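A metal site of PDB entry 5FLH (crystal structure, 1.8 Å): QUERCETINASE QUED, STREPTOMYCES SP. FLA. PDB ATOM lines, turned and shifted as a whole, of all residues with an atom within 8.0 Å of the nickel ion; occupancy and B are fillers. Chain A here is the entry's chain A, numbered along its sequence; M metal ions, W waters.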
ATOM      1  N   PHE A  56      21.426 -20.324  -1.430  1.00  0.00           N
ATOM      2  CA  PHE A  56      22.585 -20.036  -0.625  1.00  0.00           C
ATOM      3  C   PHE A  56      23.503 -21.264  -0.522  1.00  0.00           C
ATOM      4  O   PHE A  56      23.118 -22.357  -0.923  1.00  0.00           O
ATOM      5  CB  PHE A  56      22.171 -19.542   0.781  1.00  0.00           C
ATOM      6  CG  PHE A  56      21.299 -20.508   1.545  1.00  0.00           C
ATOM      7  CD1 PHE A  56      19.905 -20.488   1.416  1.00  0.00           C
ATOM      8  CD2 PHE A  56      21.855 -21.450   2.386  1.00  0.00           C
ATOM      9  CE1 PHE A  56      19.117 -21.373   2.103  1.00  0.00           C
ATOM     10  CE2 PHE A  56      21.061 -22.341   3.091  1.00  0.00           C
ATOM     11  CZ  PHE A  56      19.691 -22.304   2.953  1.00  0.00           C
ATOM     12  N   ILE A  66      25.611 -29.197  12.842  1.00  0.00           N
ATOM     13  CA  ILE A  66      24.451 -28.338  13.009  1.00  0.00           C
ATOM     14  C   ILE A  66      23.429 -29.187  13.744  1.00  0.00           C
ATOM     15  O   ILE A  66      22.896 -30.135  13.181  1.00  0.00           O
ATOM     16  CB  ILE A  66      23.884 -27.828  11.645  1.00  0.00           C
ATOM     17  CG1 ILE A  66      24.710 -26.638  11.135  1.00  0.00           C
ATOM     18  CG2 ILE A  66      22.405 -27.439  11.753  1.00  0.00           C
ATOM     19  CD1 ILE A  66      26.126 -26.967  10.706  1.00  0.00           C
ATOM     20  N   PRO A  67      23.199 -28.868  15.036  1.00  0.00           N
ATOM     21  CA  PRO A  67      22.360 -29.666  15.936  1.00  0.00           C
ATOM     22  C   PRO A  67      20.898 -29.733  15.511  1.00  0.00           C
ATOM     23  O   PRO A  67      20.444 -28.920  14.712  1.00  0.00           O
ATOM     24  CB  PRO A  67      22.490 -28.940  17.276  1.00  0.00           C
ATOM     25  CG  PRO A  67      22.833 -27.533  16.899  1.00  0.00           C
ATOM     26  CD  PRO A  67      23.707 -27.657  15.694  1.00  0.00           C
ATOM     27  N   ALA A  68      20.170 -30.698  16.077  1.00  0.00           N
ATOM     28  CA  ALA A  68      18.791 -30.978  15.714  1.00  0.00           C
ATOM     29  C   ALA A  68      17.878 -29.755  15.778  1.00  0.00           C
ATOM     30  O   ALA A  68      17.887 -28.991  16.761  1.00  0.00           O
ATOM     31  CB  ALA A  68      18.248 -32.088  16.609  1.00  0.00           C
ATOM     32  N   HIS A  69      17.107 -29.575  14.719  1.00  0.00           N
ATOM     33  CA  HIS A  69      16.084 -28.526  14.687  1.00  0.00           C
ATOM     34  C   HIS A  69      15.015 -28.875  13.678  1.00  0.00           C
ATOM     35  O   HIS A  69      15.138 -29.869  12.954  1.00  0.00           O
ATOM     36  CB  HIS A  69      16.709 -27.167  14.371  1.00  0.00           C
ATOM     37  CG  HIS A  69      17.242 -27.047  12.977  1.00  0.00           C
ATOM     38  ND1 HIS A  69      18.486 -27.516  12.622  1.00  0.00           N
ATOM     39  CD2 HIS A  69      16.706 -26.494  11.849  1.00  0.00           C
ATOM     40  CE1 HIS A  69      18.694 -27.269  11.335  1.00  0.00           C
ATOM     41  NE2 HIS A  69      17.637 -26.633  10.846  1.00  0.00           N
ATOM     42  N   SER A  70      13.953 -28.064  13.637  1.00  0.00           N
ATOM     43  CA  SER A  70      12.888 -28.253  12.664  1.00  0.00           C
ATOM     44  C   SER A  70      12.340 -26.923  12.207  1.00  0.00           C
ATOM     45  O   SER A  70      12.590 -25.877  12.824  1.00  0.00           O
ATOM     46  CB  SER A  70      11.755 -29.119  13.235  1.00  0.00           C
ATOM     47  OG  SER A  70      11.225 -28.500  14.393  1.00  0.00           O
ATOM     48  N   HIS A  71      11.610 -26.973  11.091  1.00  0.00           N
ATOM     49  CA  HIS A  71      10.988 -25.808  10.496  1.00  0.00           C
ATOM     50  C   HIS A  71       9.523 -26.133  10.300  1.00  0.00           C
ATOM     51  O   HIS A  71       9.170 -27.139   9.664  1.00  0.00           O
ATOM     52  CB  HIS A  71      11.650 -25.435   9.156  1.00  0.00           C
ATOM     53  CG  HIS A  71      13.148 -25.415   9.221  1.00  0.00           C
ATOM     54  ND1 HIS A  71      13.858 -24.408   9.839  1.00  0.00           N
ATOM     55  CD2 HIS A  71      14.071 -26.288   8.763  1.00  0.00           C
ATOM     56  CE1 HIS A  71      15.147 -24.660   9.752  1.00  0.00           C
ATOM     57  NE2 HIS A  71      15.308 -25.798   9.111  1.00  0.00           N
ATOM     58  N   THR A  74       8.759 -24.537   6.465  1.00  0.00           N
ATOM     59  CA  THR A  74       9.837 -24.400   5.485  1.00  0.00           C
ATOM     60  C   THR A  74      10.384 -25.754   5.046  1.00  0.00           C
ATOM     61  O   THR A  74      10.568 -26.649   5.874  1.00  0.00           O
ATOM     62  CB  THR A  74      10.976 -23.557   6.049  1.00  0.00           C
ATOM     63  OG1 THR A  74      10.440 -22.388   6.658  1.00  0.00           O
ATOM     64  CG2 THR A  74      11.962 -23.151   4.957  1.00  0.00           C
ATOM     65  N   TYR A  75      10.603 -25.891   3.738  1.00  0.00           N
ATOM     66  CA  TYR A  75      11.154 -27.097   3.154  1.00  0.00           C
ATOM     67  C   TYR A  75      12.589 -26.765   2.833  1.00  0.00           C
ATOM     68  O   TYR A  75      12.847 -25.636   2.408  1.00  0.00           O
ATOM     69  CB  TYR A  75      10.415 -27.519   1.892  1.00  0.00           C
ATOM     70  CG  TYR A  75       8.982 -27.901   2.130  1.00  0.00           C
ATOM     71  CD1 TYR A  75       7.985 -26.925   2.256  1.00  0.00           C
ATOM     72  CD2 TYR A  75       8.598 -29.230   2.211  1.00  0.00           C
ATOM     73  CE1 TYR A  75       6.661 -27.282   2.482  1.00  0.00           C
ATOM     74  CE2 TYR A  75       7.280 -29.589   2.449  1.00  0.00           C
ATOM     75  CZ  TYR A  75       6.314 -28.607   2.577  1.00  0.00           C
ATOM     76  OH  TYR A  75       4.997 -28.979   2.788  1.00  0.00           O
ATOM     77  N   GLU A  76      13.485 -27.722   3.047  1.00  0.00           N
ATOM     78  CA  GLU A  76      14.921 -27.481   2.927  1.00  0.00           C
ATOM     79  C   GLU A  76      15.597 -28.487   1.999  1.00  0.00           C
ATOM     80  O   GLU A  76      15.406 -29.701   2.106  1.00  0.00           O
ATOM     81  CB  GLU A  76      15.584 -27.512   4.314  1.00  0.00           C
ATOM     82  CG  GLU A  76      16.706 -26.523   4.436  1.00  0.00           C
ATOM     83  CD  GLU A  76      17.381 -26.516   5.807  1.00  0.00           C
ATOM     84  OE1 GLU A  76      16.686 -26.648   6.846  1.00  0.00           O
ATOM     85  OE2 GLU A  76      18.615 -26.354   5.827  1.00  0.00           O
ATOM     86  N   VAL A  77      16.419 -27.957   1.098  1.00  0.00           N
ATOM     87  CA  VAL A  77      17.193 -28.765   0.173  1.00  0.00           C
ATOM     88  C   VAL A  77      18.658 -28.743   0.571  1.00  0.00           C
ATOM     89  O   VAL A  77      19.177 -27.709   0.971  1.00  0.00           O
ATOM     90  CB  VAL A  77      17.068 -28.242  -1.300  1.00  0.00           C
ATOM     91  CG1 VAL A  77      18.292 -28.677  -2.149  1.00  0.00           C
ATOM     92  CG2 VAL A  77      15.776 -28.718  -1.916  1.00  0.00           C
ATOM     93  N   PHE A  78      19.290 -29.905   0.472  1.00  0.00           N
ATOM     94  CA  PHE A  78      20.737 -30.088   0.582  1.00  0.00           C
ATOM     95  C   PHE A  78      21.279 -30.664  -0.712  1.00  0.00           C
ATOM     96  O   PHE A  78      20.937 -31.791  -1.077  1.00  0.00           O
ATOM     97  CB  PHE A  78      21.093 -31.053   1.728  1.00  0.00           C
ATOM     98  CG  PHE A  78      20.846 -30.482   3.093  1.00  0.00           C
ATOM     99  CD1 PHE A  78      19.538 -30.324   3.561  1.00  0.00           C
ATOM    100  CD2 PHE A  78      21.895 -30.149   3.924  1.00  0.00           C
ATOM    101  CE1 PHE A  78      19.297 -29.787   4.827  1.00  0.00           C
ATOM    102  CE2 PHE A  78      21.658 -29.631   5.184  1.00  0.00           C
ATOM    103  CZ  PHE A  78      20.354 -29.444   5.631  1.00  0.00           C
ATOM    104  N   LEU A  87      23.691 -36.339   6.613  1.00  0.00           N
ATOM    105  CA  LEU A  87      22.439 -35.676   6.880  1.00  0.00           C
ATOM    106  C   LEU A  87      21.553 -36.637   7.652  1.00  0.00           C
ATOM    107  O   LEU A  87      21.333 -37.749   7.210  1.00  0.00           O
ATOM    108  CB  LEU A  87      21.747 -35.280   5.569  1.00  0.00           C
ATOM    109  CG  LEU A  87      20.354 -34.648   5.702  1.00  0.00           C
ATOM    110  CD1 LEU A  87      20.395 -33.341   6.479  1.00  0.00           C
ATOM    111  CD2 LEU A  87      19.755 -34.449   4.329  1.00  0.00           C
ATOM    112  N   VAL A 109      14.496 -32.210   3.230  1.00  0.00           N
ATOM    113  CA  VAL A 109      13.851 -32.167   4.535  1.00  0.00           C
ATOM    114  C   VAL A 109      12.519 -31.385   4.486  1.00  0.00           C
ATOM    115  O   VAL A 109      12.557 -30.138   4.563  1.00  0.00           O
ATOM    116  CB  VAL A 109      14.767 -31.515   5.569  1.00  0.00           C
ATOM    117  CG1 VAL A 109      14.143 -31.588   6.995  1.00  0.00           C
ATOM    118  CG2 VAL A 109      16.155 -32.171   5.548  1.00  0.00           C
ATOM    119  N   CYS A 113      10.032 -31.858  10.028  1.00  0.00           N
ATOM    120  CA  CYS A 113      10.898 -33.009  10.229  1.00  0.00           C
ATOM    121  C   CYS A 113      12.183 -32.551  10.902  1.00  0.00           C
ATOM    122  O   CYS A 113      12.829 -31.567  10.472  1.00  0.00           O
ATOM    123  CB  CYS A 113      11.184 -33.711   8.908  1.00  0.00           C
ATOM    124  SG  CYS A 113       9.704 -34.397   8.124  1.00  0.00           S
ATOM    125  N   VAL A 114      12.537 -33.206  12.002  1.00  0.00           N
ATOM    126  CA  VAL A 114      13.723 -32.781  12.721  1.00  0.00           C
ATOM    127  C   VAL A 114      14.914 -33.221  11.904  1.00  0.00           C
ATOM    128  O   VAL A 114      14.906 -34.321  11.312  1.00  0.00           O
ATOM    129  CB  VAL A 114      13.814 -33.387  14.131  1.00  0.00           C
ATOM    130  CG1 VAL A 114      15.072 -32.893  14.842  1.00  0.00           C
ATOM    131  CG2 VAL A 114      12.569 -33.018  14.938  1.00  0.00           C
ATOM    132  N   HIS A 115      15.944 -32.373  11.870  1.00  0.00           N
ATOM    133  CA  HIS A 115      17.104 -32.679  11.046  1.00  0.00           C
ATOM    134  C   HIS A 115      18.368 -32.079  11.652  1.00  0.00           C
ATOM    135  O   HIS A 115      18.334 -31.071  12.387  1.00  0.00           O
ATOM    136  CB  HIS A 115      16.858 -32.212   9.571  1.00  0.00           C
ATOM    137  CG  HIS A 115      16.579 -30.744   9.403  1.00  0.00           C
ATOM    138  ND1 HIS A 115      15.404 -30.157   9.834  1.00  0.00           N
ATOM    139  CD2 HIS A 115      17.337 -29.747   8.892  1.00  0.00           C
ATOM    140  CE1 HIS A 115      15.454 -28.857   9.591  1.00  0.00           C
ATOM    141  NE2 HIS A 115      16.622 -28.575   9.012  1.00  0.00           N
ATOM    142  N   ALA A 116      19.484 -32.735  11.345  1.00  0.00           N
ATOM    143  CA  ALA A 116      20.798 -32.239  11.686  1.00  0.00           C
ATOM    144  C   ALA A 116      21.794 -32.717  10.616  1.00  0.00           C
ATOM    145  O   ALA A 116      21.502 -33.630   9.844  1.00  0.00           O
ATOM    146  CB  ALA A 116      21.222 -32.735  13.087  1.00  0.00           C
ATOM    147  N   TYR A 117      22.961 -32.100  10.555  1.00  0.00           N
ATOM    148  CA  TYR A 117      23.985 -32.648   9.668  1.00  0.00           C
ATOM    149  C   TYR A 117      25.370 -32.395  10.201  1.00  0.00           C
ATOM    150  O   TYR A 117      25.581 -31.524  11.065  1.00  0.00           O
ATOM    151  CB  TYR A 117      23.867 -32.066   8.252  1.00  0.00           C
ATOM    152  CG  TYR A 117      23.995 -30.550   8.155  1.00  0.00           C
ATOM    153  CD1 TYR A 117      22.864 -29.737   8.281  1.00  0.00           C
ATOM    154  CD2 TYR A 117      25.216 -29.955   7.915  1.00  0.00           C
ATOM    155  CE1 TYR A 117      22.959 -28.370   8.164  1.00  0.00           C
ATOM    156  CE2 TYR A 117      25.319 -28.577   7.804  1.00  0.00           C
ATOM    157  CZ  TYR A 117      24.194 -27.793   7.922  1.00  0.00           C
ATOM    158  OH  TYR A 117      24.275 -26.421   7.814  1.00  0.00           O
ATOM    159  N   ALA A 130      15.789 -22.899   1.106  1.00  0.00           N
ATOM    160  CA  ALA A 130      14.968 -23.070   2.301  1.00  0.00           C
ATOM    161  C   ALA A 130      13.775 -22.131   2.208  1.00  0.00           C
ATOM    162  O   ALA A 130      13.895 -20.940   2.458  1.00  0.00           O
ATOM    163  CB  ALA A 130      15.770 -22.797   3.574  1.00  0.00           C
ATOM    164  N   PHE A 137      13.789 -18.108   4.338  1.00  0.00           N
ATOM    165  CA  PHE A 137      14.434 -18.369   5.626  1.00  0.00           C
ATOM    166  C   PHE A 137      15.824 -17.737   5.774  1.00  0.00           C
ATOM    167  O   PHE A 137      16.372 -17.658   6.886  1.00  0.00           O
ATOM    168  CB  PHE A 137      14.494 -19.915   5.773  1.00  0.00           C
ATOM    169  CG  PHE A 137      15.033 -20.407   7.090  1.00  0.00           C
ATOM    170  CD1 PHE A 137      14.250 -20.344   8.236  1.00  0.00           C
ATOM    171  CD2 PHE A 137      16.292 -20.978   7.168  1.00  0.00           C
ATOM    172  CE1 PHE A 137      14.747 -20.803   9.451  1.00  0.00           C
ATOM    173  CE2 PHE A 137      16.788 -21.441   8.360  1.00  0.00           C
ATOM    174  CZ  PHE A 137      16.023 -21.354   9.509  1.00  0.00           C
ATOM    175  N   PHE A 140      18.086 -15.687   8.511  1.00  0.00           N
ATOM    176  CA  PHE A 140      18.250 -16.322   9.812  1.00  0.00           C
ATOM    177  C   PHE A 140      19.709 -16.433  10.262  1.00  0.00           C
ATOM    178  O   PHE A 140      20.032 -16.212  11.430  1.00  0.00           O
ATOM    179  CB  PHE A 140      17.626 -17.715   9.772  1.00  0.00           C
ATOM    180  CG  PHE A 140      18.181 -18.659  10.801  1.00  0.00           C
ATOM    181  CD1 PHE A 140      17.785 -18.591  12.117  1.00  0.00           C
ATOM    182  CD2 PHE A 140      19.085 -19.646  10.429  1.00  0.00           C
ATOM    183  CE1 PHE A 140      18.297 -19.468  13.067  1.00  0.00           C
ATOM    184  CE2 PHE A 140      19.597 -20.536  11.353  1.00  0.00           C
ATOM    185  CZ  PHE A 140      19.205 -20.439  12.680  1.00  0.00           C
ATOM    186  N   PHE A 141      20.600 -16.783   9.336  1.00  0.00           N
ATOM    187  CA  PHE A 141      21.965 -17.117   9.688  1.00  0.00           C
ATOM    188  C   PHE A 141      22.681 -15.907  10.236  1.00  0.00           C
ATOM    189  O   PHE A 141      23.391 -16.007  11.236  1.00  0.00           O
ATOM    190  CB  PHE A 141      22.695 -17.697   8.464  1.00  0.00           C
ATOM    191  CG  PHE A 141      22.051 -18.952   7.934  1.00  0.00           C
ATOM    192  CD1 PHE A 141      22.325 -20.178   8.507  1.00  0.00           C
ATOM    193  CD2 PHE A 141      21.134 -18.892   6.898  1.00  0.00           C
ATOM    194  CE1 PHE A 141      21.703 -21.340   8.040  1.00  0.00           C
ATOM    195  CE2 PHE A 141      20.516 -20.038   6.415  1.00  0.00           C
ATOM    196  CZ  PHE A 141      20.808 -21.263   6.994  1.00  0.00           C
ATOM    197  N   ASP A 173      11.672 -19.395  10.917  1.00  0.00           N
ATOM    198  CA  ASP A 173      10.880 -20.582  11.151  1.00  0.00           C
ATOM    199  C   ASP A 173      11.791 -21.718  11.583  1.00  0.00           C
ATOM    200  O   ASP A 173      11.908 -22.740  10.915  1.00  0.00           O
ATOM    201  CB  ASP A 173      10.100 -20.929   9.892  1.00  0.00           C
ATOM    202  CG  ASP A 173       9.345 -22.228  10.021  1.00  0.00           C
ATOM    203  OD1 ASP A 173       9.005 -22.635  11.153  1.00  0.00           O
ATOM    204  OD2 ASP A 173       9.133 -22.855   8.977  1.00  0.00           O
ATOM    205  N   VAL A 174      12.435 -21.556  12.733  1.00  0.00           N
ATOM    206  CA  VAL A 174      13.296 -22.611  13.255  1.00  0.00           C
ATOM    207  C   VAL A 174      13.052 -22.869  14.737  1.00  0.00           C
ATOM    208  O   VAL A 174      13.123 -21.951  15.562  1.00  0.00           O
ATOM    209  CB  VAL A 174      14.793 -22.306  13.033  1.00  0.00           C
ATOM    210  CG1 VAL A 174      15.188 -20.989  13.649  1.00  0.00           C
ATOM    211  CG2 VAL A 174      15.651 -23.434  13.584  1.00  0.00           C
HETATM  212 NI    NI M   1      17.143 -26.653   8.841  1.00  0.00          NI
HETATM  213  O   HOH W   1      18.060 -24.773   8.826  1.00  0.00           O
HETATM  214  O   HOH W   2      19.068 -27.126   8.336  1.00  0.00           O
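O of Cys 113 is in hydrogen-bond range of ND1 of His 115.
ND1 of His 71 is in hydrogen-bond range of O of Asp 173, at 2.8 Å.
The backbone NH (N) of Val 109 sits at hydrogen-bond distance from the backbone carbonyl oxygen (O) of Glu 76 (2.9 Å).
The backbone carbonyl oxygen of Pro 67 is in hydrogen-bond range of a ring nitrogen (ND1) of His 69.
Four residues have an atom within 4 Å of the nickel ion: His 69, His 71, Glu 76 and His 115.
The nickel ion is bound by NE2 of His 115 (2.0 Å), NE2 of His 71 (2.0 Å), water W2 (2.0 Å), OE1 of Glu 76 (2.0 Å), NE2 of His 69 (2.1 Å) and water W1 (2.1 Å).
The nickel ion has six donor atoms within binding distance.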
